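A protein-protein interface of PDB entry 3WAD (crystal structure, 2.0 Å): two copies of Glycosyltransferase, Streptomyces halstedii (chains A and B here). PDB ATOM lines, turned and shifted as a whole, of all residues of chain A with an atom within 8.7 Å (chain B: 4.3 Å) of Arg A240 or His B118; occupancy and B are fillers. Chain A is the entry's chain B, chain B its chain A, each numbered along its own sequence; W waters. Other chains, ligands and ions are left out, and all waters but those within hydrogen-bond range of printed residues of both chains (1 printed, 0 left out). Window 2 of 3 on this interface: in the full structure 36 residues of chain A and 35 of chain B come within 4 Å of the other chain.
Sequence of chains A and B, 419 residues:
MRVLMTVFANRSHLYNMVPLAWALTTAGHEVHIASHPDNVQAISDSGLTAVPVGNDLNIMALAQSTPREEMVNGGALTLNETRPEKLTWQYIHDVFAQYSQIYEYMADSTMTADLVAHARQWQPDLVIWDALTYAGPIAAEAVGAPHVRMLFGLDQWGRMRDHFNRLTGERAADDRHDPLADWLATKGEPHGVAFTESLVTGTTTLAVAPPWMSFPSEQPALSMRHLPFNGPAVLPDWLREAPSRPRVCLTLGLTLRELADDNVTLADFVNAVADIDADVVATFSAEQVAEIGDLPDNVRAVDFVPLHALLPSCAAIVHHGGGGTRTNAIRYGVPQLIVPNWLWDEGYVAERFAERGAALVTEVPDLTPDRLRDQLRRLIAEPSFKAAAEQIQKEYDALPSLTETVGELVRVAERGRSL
The backbone carbonyl oxygen (O) of Pro B52 sits at hydrogen-bond distance from the guanidinium group (NH2) of Arg A240 (3.1 Å).
A ring nitrogen (ND1) of His B32 sits at hydrogen-bond distance from a ring nitrogen (NE2) of His B118 (2.9 Å). OD2 of Asp A237 is in salt-bridge range of NE of Arg A240 (3.9 Å).
Among the printed residues, merely in contact across the chains: Leu A235 with His B32 (3.9 Å), Leu A235 with Val B51 (3.9 Å), Leu A235 with Pro B52 (3.9 Å), Leu A235 with His B118 (3.9 Å), Arg A240 with His B118 (3.8 Å), Arg A240 with Gln B121 (3.2 Å) and Ala A242 with Gln B121 (3.3 Å).
Trp A238 touches none of the printed residues of chain B. Of the printed residues of chain B, Arg A240 touches Pro B52 (3.1 Å), His B118 (3.8 Å) and Gln B121 (3.2 Å). Of the printed residues of chain B, Ala A242 touches Gln B121. Printed residues of chain A within 4 Å of His B32: Leu A235 (3.9 Å). Ala B117 touches none of the printed residues of chain A. His B118 touches just these residues of chain A: Leu A235 (3.9 Å) and Arg A240 (3.8 Å). No residue of chain A comes within 4 Å of Ala B119. The nearest printed residue of chain B that does not touch Arg A240 is Val B51 (4.01 Å).
Of the 13 printed residues of chain B, 5 touch a printed residue of chain A. Printed residues of chain B that touch a printed residue of chain A: His B32, Val B51, Pro B52, His B118 and Gln B121. Hydrophobic or aromatic side chains of chain B within 4 Å of the printed part of chain A: His B32, Val B51, Pro B52 and His B118. Printed residues of chain A that touch a printed residue of chain B: Leu A235, Arg A240 and Ala A242. Along chain A the printed residues that touch a printed residue of chain B span positions 235 to 242. Among the printed residues, 8 pairs touch across the chains.
No position is printed for both chains.
Water W1 lies within hydrogen-bond range of NH1 of Arg A240 (2.8 Å) and O of Asp B114 (2.8 Å).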
ATOM      1  N   VAL A 234     -19.195  25.922 -11.624  1.00  0.00           N
ATOM      2  CA  VAL A 234     -19.341  25.889 -13.091  1.00  0.00           C
ATOM      3  C   VAL A 234     -20.262  24.705 -13.412  1.00  0.00           C
ATOM      4  O   VAL A 234     -20.051  23.594 -12.912  1.00  0.00           O
ATOM      5  CB  VAL A 234     -17.998  25.705 -13.773  1.00  0.00           C
ATOM      6  CG1 VAL A 234     -18.164  25.653 -15.301  1.00  0.00           C
ATOM      7  CG2 VAL A 234     -17.044  26.847 -13.344  1.00  0.00           C
ATOM      8  N   LEU A 235     -21.337  24.928 -14.141  1.00  0.00           N
ATOM      9  CA  LEU A 235     -22.256  23.839 -14.401  1.00  0.00           C
ATOM     10  C   LEU A 235     -21.603  22.894 -15.401  1.00  0.00           C
ATOM     11  O   LEU A 235     -21.258  23.351 -16.474  1.00  0.00           O
ATOM     12  CB  LEU A 235     -23.520  24.378 -15.001  1.00  0.00           C
ATOM     13  CG  LEU A 235     -24.827  23.867 -14.435  1.00  0.00           C
ATOM     14  CD1 LEU A 235     -24.976  24.581 -13.070  1.00  0.00           C
ATOM     15  CD2 LEU A 235     -25.976  24.228 -15.420  1.00  0.00           C
ATOM     16  N   PRO A 236     -21.384  21.603 -15.041  1.00  0.00           N
ATOM     17  CA  PRO A 236     -20.808  20.715 -16.069  1.00  0.00           C
ATOM     18  C   PRO A 236     -21.856  20.284 -17.097  1.00  0.00           C
ATOM     19  O   PRO A 236     -23.074  20.349 -16.833  1.00  0.00           O
ATOM     20  CB  PRO A 236     -20.274  19.525 -15.264  1.00  0.00           C
ATOM     21  CG  PRO A 236     -21.221  19.414 -14.115  1.00  0.00           C
ATOM     22  CD  PRO A 236     -21.614  20.880 -13.777  1.00  0.00           C
ATOM     23  N   ASP A 237     -21.385  19.869 -18.267  1.00  0.00           N
ATOM     24  CA  ASP A 237     -22.273  19.520 -19.356  1.00  0.00           C
ATOM     25  C   ASP A 237     -23.255  18.454 -18.914  1.00  0.00           C
ATOM     26  O   ASP A 237     -24.439  18.502 -19.200  1.00  0.00           O
ATOM     27  CB  ASP A 237     -21.453  18.967 -20.517  1.00  0.00           C
ATOM     28  CG  ASP A 237     -21.010  20.045 -21.494  1.00  0.00           C
ATOM     29  OD1 ASP A 237     -20.093  19.802 -22.316  1.00  0.00           O
ATOM     30  OD2 ASP A 237     -21.586  21.142 -21.464  1.00  0.00           O
ATOM     31  N   TRP A 238     -22.756  17.478 -18.193  1.00  0.00           N
ATOM     32  CA  TRP A 238     -23.558  16.318 -17.898  1.00  0.00           C
ATOM     33  C   TRP A 238     -24.748  16.656 -16.971  1.00  0.00           C
ATOM     34  O   TRP A 238     -25.824  16.055 -17.107  1.00  0.00           O
ATOM     35  CB  TRP A 238     -22.645  15.205 -17.374  1.00  0.00           C
ATOM     36  CG  TRP A 238     -22.032  15.533 -16.104  1.00  0.00           C
ATOM     37  CD1 TRP A 238     -20.749  15.981 -15.877  1.00  0.00           C
ATOM     38  CD2 TRP A 238     -22.676  15.466 -14.826  1.00  0.00           C
ATOM     39  NE1 TRP A 238     -20.564  16.180 -14.524  1.00  0.00           N
ATOM     40  CE2 TRP A 238     -21.732  15.875 -13.863  1.00  0.00           C
ATOM     41  CE3 TRP A 238     -23.969  15.086 -14.405  1.00  0.00           C
ATOM     42  CZ2 TRP A 238     -22.028  15.914 -12.507  1.00  0.00           C
ATOM     43  CZ3 TRP A 238     -24.266  15.127 -13.065  1.00  0.00           C
ATOM     44  CH2 TRP A 238     -23.289  15.540 -12.125  1.00  0.00           C
ATOM     45  N   LEU A 239     -24.574  17.637 -16.065  1.00  0.00           N
ATOM     46  CA  LEU A 239     -25.697  18.210 -15.288  1.00  0.00           C
ATOM     47  C   LEU A 239     -26.719  18.964 -16.135  1.00  0.00           C
ATOM     48  O   LEU A 239     -27.837  19.230 -15.694  1.00  0.00           O
ATOM     49  CB  LEU A 239     -25.213  19.142 -14.177  1.00  0.00           C
ATOM     50  CG  LEU A 239     -25.179  18.582 -12.759  1.00  0.00           C
ATOM     51  CD1 LEU A 239     -24.705  19.599 -11.783  1.00  0.00           C
ATOM     52  CD2 LEU A 239     -26.544  18.088 -12.377  1.00  0.00           C
ATOM     53  N   ARG A 240     -26.353  19.332 -17.346  1.00  0.00           N
ATOM     54  CA  ARG A 240     -27.213  20.227 -18.102  1.00  0.00           C
ATOM     55  C   ARG A 240     -28.301  19.442 -18.808  1.00  0.00           C
ATOM     56  O   ARG A 240     -29.343  19.999 -19.175  1.00  0.00           O
ATOM     57  CB  ARG A 240     -26.395  21.115 -19.058  1.00  0.00           C
ATOM     58  CG  ARG A 240     -25.934  22.418 -18.379  1.00  0.00           C
ATOM     59  CD  ARG A 240     -24.430  22.751 -18.606  1.00  0.00           C
ATOM     60  NE  ARG A 240     -24.068  23.581 -19.775  1.00  0.00           N
ATOM     61  CZ  ARG A 240     -24.864  23.948 -20.790  1.00  0.00           C
ATOM     62  NH1 ARG A 240     -26.139  23.566 -20.873  1.00  0.00           N
ATOM     63  NH2 ARG A 240     -24.371  24.731 -21.747  1.00  0.00           N
ATOM     64  N   GLU A 241     -28.075  18.137 -18.937  1.00  0.00           N
ATOM     65  CA  GLU A 241     -28.956  17.239 -19.672  1.00  0.00           C
ATOM     66  C   GLU A 241     -30.132  16.747 -18.825  1.00  0.00           C
ATOM     67  O   GLU A 241     -29.949  16.282 -17.695  1.00  0.00           O
ATOM     68  CB  GLU A 241     -28.160  16.027 -20.183  1.00  0.00           C
ATOM     69  CG  GLU A 241     -26.770  16.364 -20.789  1.00  0.00           C
ATOM     70  CD  GLU A 241     -25.964  15.119 -21.220  1.00  0.00           C
ATOM     71  OE1 GLU A 241     -26.480  13.984 -21.091  1.00  0.00           O
ATOM     72  OE2 GLU A 241     -24.813  15.269 -21.704  1.00  0.00           O
ATOM     73  N   ALA A 242     -31.343  16.837 -19.380  1.00  0.00           N
ATOM     74  CA  ALA A 242     -32.527  16.145 -18.835  1.00  0.00           C
ATOM     75  C   ALA A 242     -32.153  14.912 -17.985  1.00  0.00           C
ATOM     76  O   ALA A 242     -31.479  13.983 -18.455  1.00  0.00           O
ATOM     77  CB  ALA A 242     -33.471  15.745 -19.976  1.00  0.00           C
ATOM     78  N   PRO A 243     -32.556  14.916 -16.717  1.00  0.00           N
ATOM     79  CA  PRO A 243     -32.294  13.746 -15.886  1.00  0.00           C
ATOM     80  C   PRO A 243     -32.930  12.470 -16.463  1.00  0.00           C
ATOM     81  O   PRO A 243     -34.134  12.414 -16.696  1.00  0.00           O
ATOM     82  CB  PRO A 243     -32.911  14.127 -14.533  1.00  0.00           C
ATOM     83  CG  PRO A 243     -33.827  15.310 -14.834  1.00  0.00           C
ATOM     84  CD  PRO A 243     -33.145  16.028 -15.951  1.00  0.00           C
ATOM     85  N   ARG A 247     -31.710  10.006  -9.201  1.00  0.00           N
ATOM     86  CA  ARG A 247     -30.279  10.264  -8.987  1.00  0.00           C
ATOM     87  C   ARG A 247     -30.055  10.178  -7.502  1.00  0.00           C
ATOM     88  O   ARG A 247     -30.964  10.485  -6.728  1.00  0.00           O
ATOM     89  CB  ARG A 247     -29.947  11.671  -9.399  1.00  0.00           C
ATOM     90  CG  ARG A 247     -28.800  11.809 -10.276  1.00  0.00           C
ATOM     91  CD  ARG A 247     -28.970  13.106 -11.053  1.00  0.00           C
ATOM     92  NE  ARG A 247     -28.764  12.882 -12.487  1.00  0.00           N
ATOM     93  CZ  ARG A 247     -28.765  13.817 -13.438  1.00  0.00           C
ATOM     94  NH1 ARG A 247     -28.929  15.100 -13.154  1.00  0.00           N
ATOM     95  NH2 ARG A 247     -28.566  13.446 -14.680  1.00  0.00           N
ATOM     96  N   ARG A 300     -21.235   7.889 -11.624  1.00  0.00           N
ATOM     97  CA  ARG A 300     -20.295   8.917 -12.127  1.00  0.00           C
ATOM     98  C   ARG A 300     -19.414   9.463 -11.033  1.00  0.00           C
ATOM     99  O   ARG A 300     -19.904  10.005 -10.025  1.00  0.00           O
ATOM    100  CB  ARG A 300     -21.045  10.082 -12.786  1.00  0.00           C
ATOM    101  CG  ARG A 300     -20.116  11.244 -13.198  1.00  0.00           C
ATOM    102  CD  ARG A 300     -20.930  12.427 -13.731  1.00  0.00           C
ATOM    103  NE  ARG A 300     -21.993  12.009 -14.653  1.00  0.00           N
ATOM    104  CZ  ARG A 300     -21.855  11.974 -15.995  1.00  0.00           C
ATOM    105  NH1 ARG A 300     -20.720  12.350 -16.590  1.00  0.00           N
ATOM    106  NH2 ARG A 300     -22.858  11.566 -16.760  1.00  0.00           N
ATOM    107  N   ALA A 309     -26.901  22.663  -7.830  1.00  0.00           N
ATOM    108  CA  ALA A 309     -27.338  22.276  -9.241  1.00  0.00           C
ATOM    109  C   ALA A 309     -27.780  20.833  -9.331  1.00  0.00           C
ATOM    110  O   ALA A 309     -28.724  20.502 -10.086  1.00  0.00           O
ATOM    111  CB  ALA A 309     -26.282  22.534 -10.303  1.00  0.00           C
ATOM    112  N   LEU B   4     -31.981  33.304 -15.302  1.00  0.00           N
ATOM    113  CA  LEU B   4     -30.871  33.137 -16.205  1.00  0.00           C
ATOM    114  C   LEU B   4     -30.357  34.523 -16.601  1.00  0.00           C
ATOM    115  O   LEU B   4     -31.067  35.283 -17.281  1.00  0.00           O
ATOM    116  CB  LEU B   4     -31.323  32.382 -17.416  1.00  0.00           C
ATOM    117  CG  LEU B   4     -30.342  32.320 -18.584  1.00  0.00           C
ATOM    118  CD1 LEU B   4     -28.999  31.670 -18.101  1.00  0.00           C
ATOM    119  CD2 LEU B   4     -30.935  31.572 -19.732  1.00  0.00           C
ATOM    120  N   HIS B  32     -28.340  31.572 -12.569  1.00  0.00           N
ATOM    121  CA  HIS B  32     -27.216  31.135 -13.456  1.00  0.00           C
ATOM    122  C   HIS B  32     -26.670  32.337 -14.228  1.00  0.00           C
ATOM    123  O   HIS B  32     -27.460  33.165 -14.718  1.00  0.00           O
ATOM    124  CB  HIS B  32     -27.661  30.101 -14.487  1.00  0.00           C
ATOM    125  CG  HIS B  32     -27.967  28.744 -13.912  1.00  0.00           C
ATOM    126  ND1 HIS B  32     -28.515  27.730 -14.672  1.00  0.00           N
ATOM    127  CD2 HIS B  32     -27.860  28.257 -12.661  1.00  0.00           C
ATOM    128  CE1 HIS B  32     -28.690  26.656 -13.917  1.00  0.00           C
ATOM    129  NE2 HIS B  32     -28.321  26.956 -12.687  1.00  0.00           N
ATOM    130  N   VAL B  51     -22.525  29.203 -16.376  1.00  0.00           N
ATOM    131  CA  VAL B  51     -22.988  28.306 -17.402  1.00  0.00           C
ATOM    132  C   VAL B  51     -22.245  28.713 -18.652  1.00  0.00           C
ATOM    133  O   VAL B  51     -22.503  29.789 -19.218  1.00  0.00           O
ATOM    134  CB  VAL B  51     -24.557  28.376 -17.662  1.00  0.00           C
ATOM    135  CG1 VAL B  51     -24.933  27.477 -18.879  1.00  0.00           C
ATOM    136  CG2 VAL B  51     -25.317  27.906 -16.439  1.00  0.00           C
ATOM    137  N   PRO B  52     -21.283  27.866 -19.106  1.00  0.00           N
ATOM    138  CA  PRO B  52     -20.580  28.196 -20.380  1.00  0.00           C
ATOM    139  C   PRO B  52     -21.487  28.026 -21.559  1.00  0.00           C
ATOM    140  O   PRO B  52     -22.317  27.090 -21.582  1.00  0.00           O
ATOM    141  CB  PRO B  52     -19.369  27.215 -20.438  1.00  0.00           C
ATOM    142  CG  PRO B  52     -19.363  26.464 -19.113  1.00  0.00           C
ATOM    143  CD  PRO B  52     -20.676  26.735 -18.368  1.00  0.00           C
ATOM    144  N   ASP B 114     -26.575  27.777 -27.805  1.00  0.00           N
ATOM    145  CA  ASP B 114     -26.327  27.121 -26.525  1.00  0.00           C
ATOM    146  C   ASP B 114     -27.164  27.726 -25.384  1.00  0.00           C
ATOM    147  O   ASP B 114     -27.581  27.005 -24.468  1.00  0.00           O
ATOM    148  CB  ASP B 114     -24.845  27.178 -26.100  1.00  0.00           C
ATOM    149  CG  ASP B 114     -23.904  26.414 -27.057  1.00  0.00           C
ATOM    150  OD1 ASP B 114     -24.374  25.589 -27.867  1.00  0.00           O
ATOM    151  OD2 ASP B 114     -22.677  26.685 -27.030  1.00  0.00           O
ATOM    152  N   LEU B 115     -27.347  29.040 -25.412  1.00  0.00           N
ATOM    153  CA  LEU B 115     -28.130  29.709 -24.361  1.00  0.00           C
ATOM    154  C   LEU B 115     -29.623  29.383 -24.545  1.00  0.00           C
ATOM    155  O   LEU B 115     -30.357  29.229 -23.583  1.00  0.00           O
ATOM    156  CB  LEU B 115     -27.957  31.233 -24.434  1.00  0.00           C
ATOM    157  CG  LEU B 115     -28.678  32.021 -23.342  1.00  0.00           C
ATOM    158  CD1 LEU B 115     -27.900  31.845 -22.076  1.00  0.00           C
ATOM    159  CD2 LEU B 115     -28.662  33.507 -23.669  1.00  0.00           C
ATOM    160  N   VAL B 116     -30.073  29.284 -25.782  1.00  0.00           N
ATOM    161  CA  VAL B 116     -31.463  28.839 -26.013  1.00  0.00           C
ATOM    162  C   VAL B 116     -31.726  27.412 -25.497  1.00  0.00           C
ATOM    163  O   VAL B 116     -32.797  27.114 -24.901  1.00  0.00           O
ATOM    164  CB  VAL B 116     -31.913  28.976 -27.499  1.00  0.00           C
ATOM    165  CG1 VAL B 116     -33.166  28.152 -27.767  1.00  0.00           C
ATOM    166  CG2 VAL B 116     -32.176  30.397 -27.845  1.00  0.00           C
ATOM    167  N   ALA B 117     -30.748  26.533 -25.717  1.00  0.00           N
ATOM    168  CA  ALA B 117     -30.903  25.132 -25.331  1.00  0.00           C
ATOM    169  C   ALA B 117     -30.895  25.006 -23.815  1.00  0.00           C
ATOM    170  O   ALA B 117     -31.791  24.355 -23.259  1.00  0.00           O
ATOM    171  CB  ALA B 117     -29.821  24.217 -26.017  1.00  0.00           C
ATOM    172  N   HIS B 118     -29.942  25.693 -23.136  1.00  0.00           N
ATOM    173  CA  HIS B 118     -29.985  25.812 -21.683  1.00  0.00           C
ATOM    174  C   HIS B 118     -31.350  26.331 -21.136  1.00  0.00           C
ATOM    175  O   HIS B 118     -31.930  25.754 -20.172  1.00  0.00           O
ATOM    176  CB  HIS B 118     -28.859  26.695 -21.160  1.00  0.00           C
ATOM    177  CG  HIS B 118     -28.833  26.748 -19.676  1.00  0.00           C
ATOM    178  ND1 HIS B 118     -28.600  25.630 -18.912  1.00  0.00           N
ATOM    179  CD2 HIS B 118     -29.076  27.757 -18.807  1.00  0.00           C
ATOM    180  CE1 HIS B 118     -28.686  25.946 -17.631  1.00  0.00           C
ATOM    181  NE2 HIS B 118     -28.952  27.238 -17.540  1.00  0.00           N
ATOM    182  N   ALA B 119     -31.861  27.418 -21.740  1.00  0.00           N
ATOM    183  CA  ALA B 119     -33.173  27.968 -21.318  1.00  0.00           C
ATOM    184  C   ALA B 119     -34.282  26.913 -21.495  1.00  0.00           C
ATOM    185  O   ALA B 119     -35.079  26.713 -20.591  1.00  0.00           O
ATOM    186  CB  ALA B 119     -33.515  29.220 -22.061  1.00  0.00           C
ATOM    187  N   ARG B 120     -34.294  26.227 -22.634  1.00  0.00           N
ATOM    188  CA  ARG B 120     -35.298  25.192 -22.903  1.00  0.00           C
ATOM    189  C   ARG B 120     -35.283  24.134 -21.825  1.00  0.00           C
ATOM    190  O   ARG B 120     -36.307  23.829 -21.258  1.00  0.00           O
ATOM    191  CB  ARG B 120     -35.120  24.581 -24.281  1.00  0.00           C
ATOM    192  CG  ARG B 120     -35.825  25.374 -25.378  1.00  0.00           C
ATOM    193  CD  ARG B 120     -35.740  24.642 -26.733  1.00  0.00           C
ATOM    194  NE  ARG B 120     -35.889  25.574 -27.850  1.00  0.00           N
ATOM    195  CZ  ARG B 120     -36.964  26.333 -28.014  1.00  0.00           C
ATOM    196  NH1 ARG B 120     -37.957  26.272 -27.117  1.00  0.00           N
ATOM    197  NH2 ARG B 120     -37.027  27.184 -29.031  1.00  0.00           N
ATOM    198  N   GLN B 121     -34.096  23.620 -21.489  1.00  0.00           N
ATOM    199  CA  GLN B 121     -33.951  22.692 -20.370  1.00  0.00           C
ATOM    200  C   GLN B 121     -34.226  23.274 -18.955  1.00  0.00           C
ATOM    201  O   GLN B 121     -34.986  22.700 -18.172  1.00  0.00           O
ATOM    202  CB  GLN B 121     -32.606  22.003 -20.478  1.00  0.00           C
ATOM    203  CG  GLN B 121     -32.418  20.857 -19.551  1.00  0.00           C
ATOM    204  CD  GLN B 121     -33.422  19.704 -19.770  1.00  0.00           C
ATOM    205  OE1 GLN B 121     -33.750  19.328 -20.914  1.00  0.00           O
ATOM    206  NE2 GLN B 121     -33.903  19.133 -18.657  1.00  0.00           N
ATOM    207  N   TRP B 122     -33.686  24.440 -18.626  1.00  0.00           N
ATOM    208  CA  TRP B 122     -33.704  24.877 -17.230  1.00  0.00           C
ATOM    209  C   TRP B 122     -34.958  25.665 -16.867  1.00  0.00           C
ATOM    210  O   TRP B 122     -35.278  25.843 -15.655  1.00  0.00           O
ATOM    211  CB  TRP B 122     -32.440  25.688 -16.918  1.00  0.00           C
ATOM    212  CG  TRP B 122     -32.246  26.037 -15.513  1.00  0.00           C
ATOM    213  CD1 TRP B 122     -32.153  25.177 -14.473  1.00  0.00           C
ATOM    214  CD2 TRP B 122     -32.002  27.370 -14.945  1.00  0.00           C
ATOM    215  NE1 TRP B 122     -31.934  25.862 -13.298  1.00  0.00           N
ATOM    216  CE2 TRP B 122     -31.827  27.201 -13.551  1.00  0.00           C
ATOM    217  CE3 TRP B 122     -31.931  28.664 -15.483  1.00  0.00           C
ATOM    218  CZ2 TRP B 122     -31.576  28.279 -12.666  1.00  0.00           C
ATOM    219  CZ3 TRP B 122     -31.684  29.752 -14.616  1.00  0.00           C
ATOM    220  CH2 TRP B 122     -31.484  29.543 -13.216  1.00  0.00           C
HETATM  221  O   HOH W   1     -26.611  24.634 -23.388  1.00  0.00           O
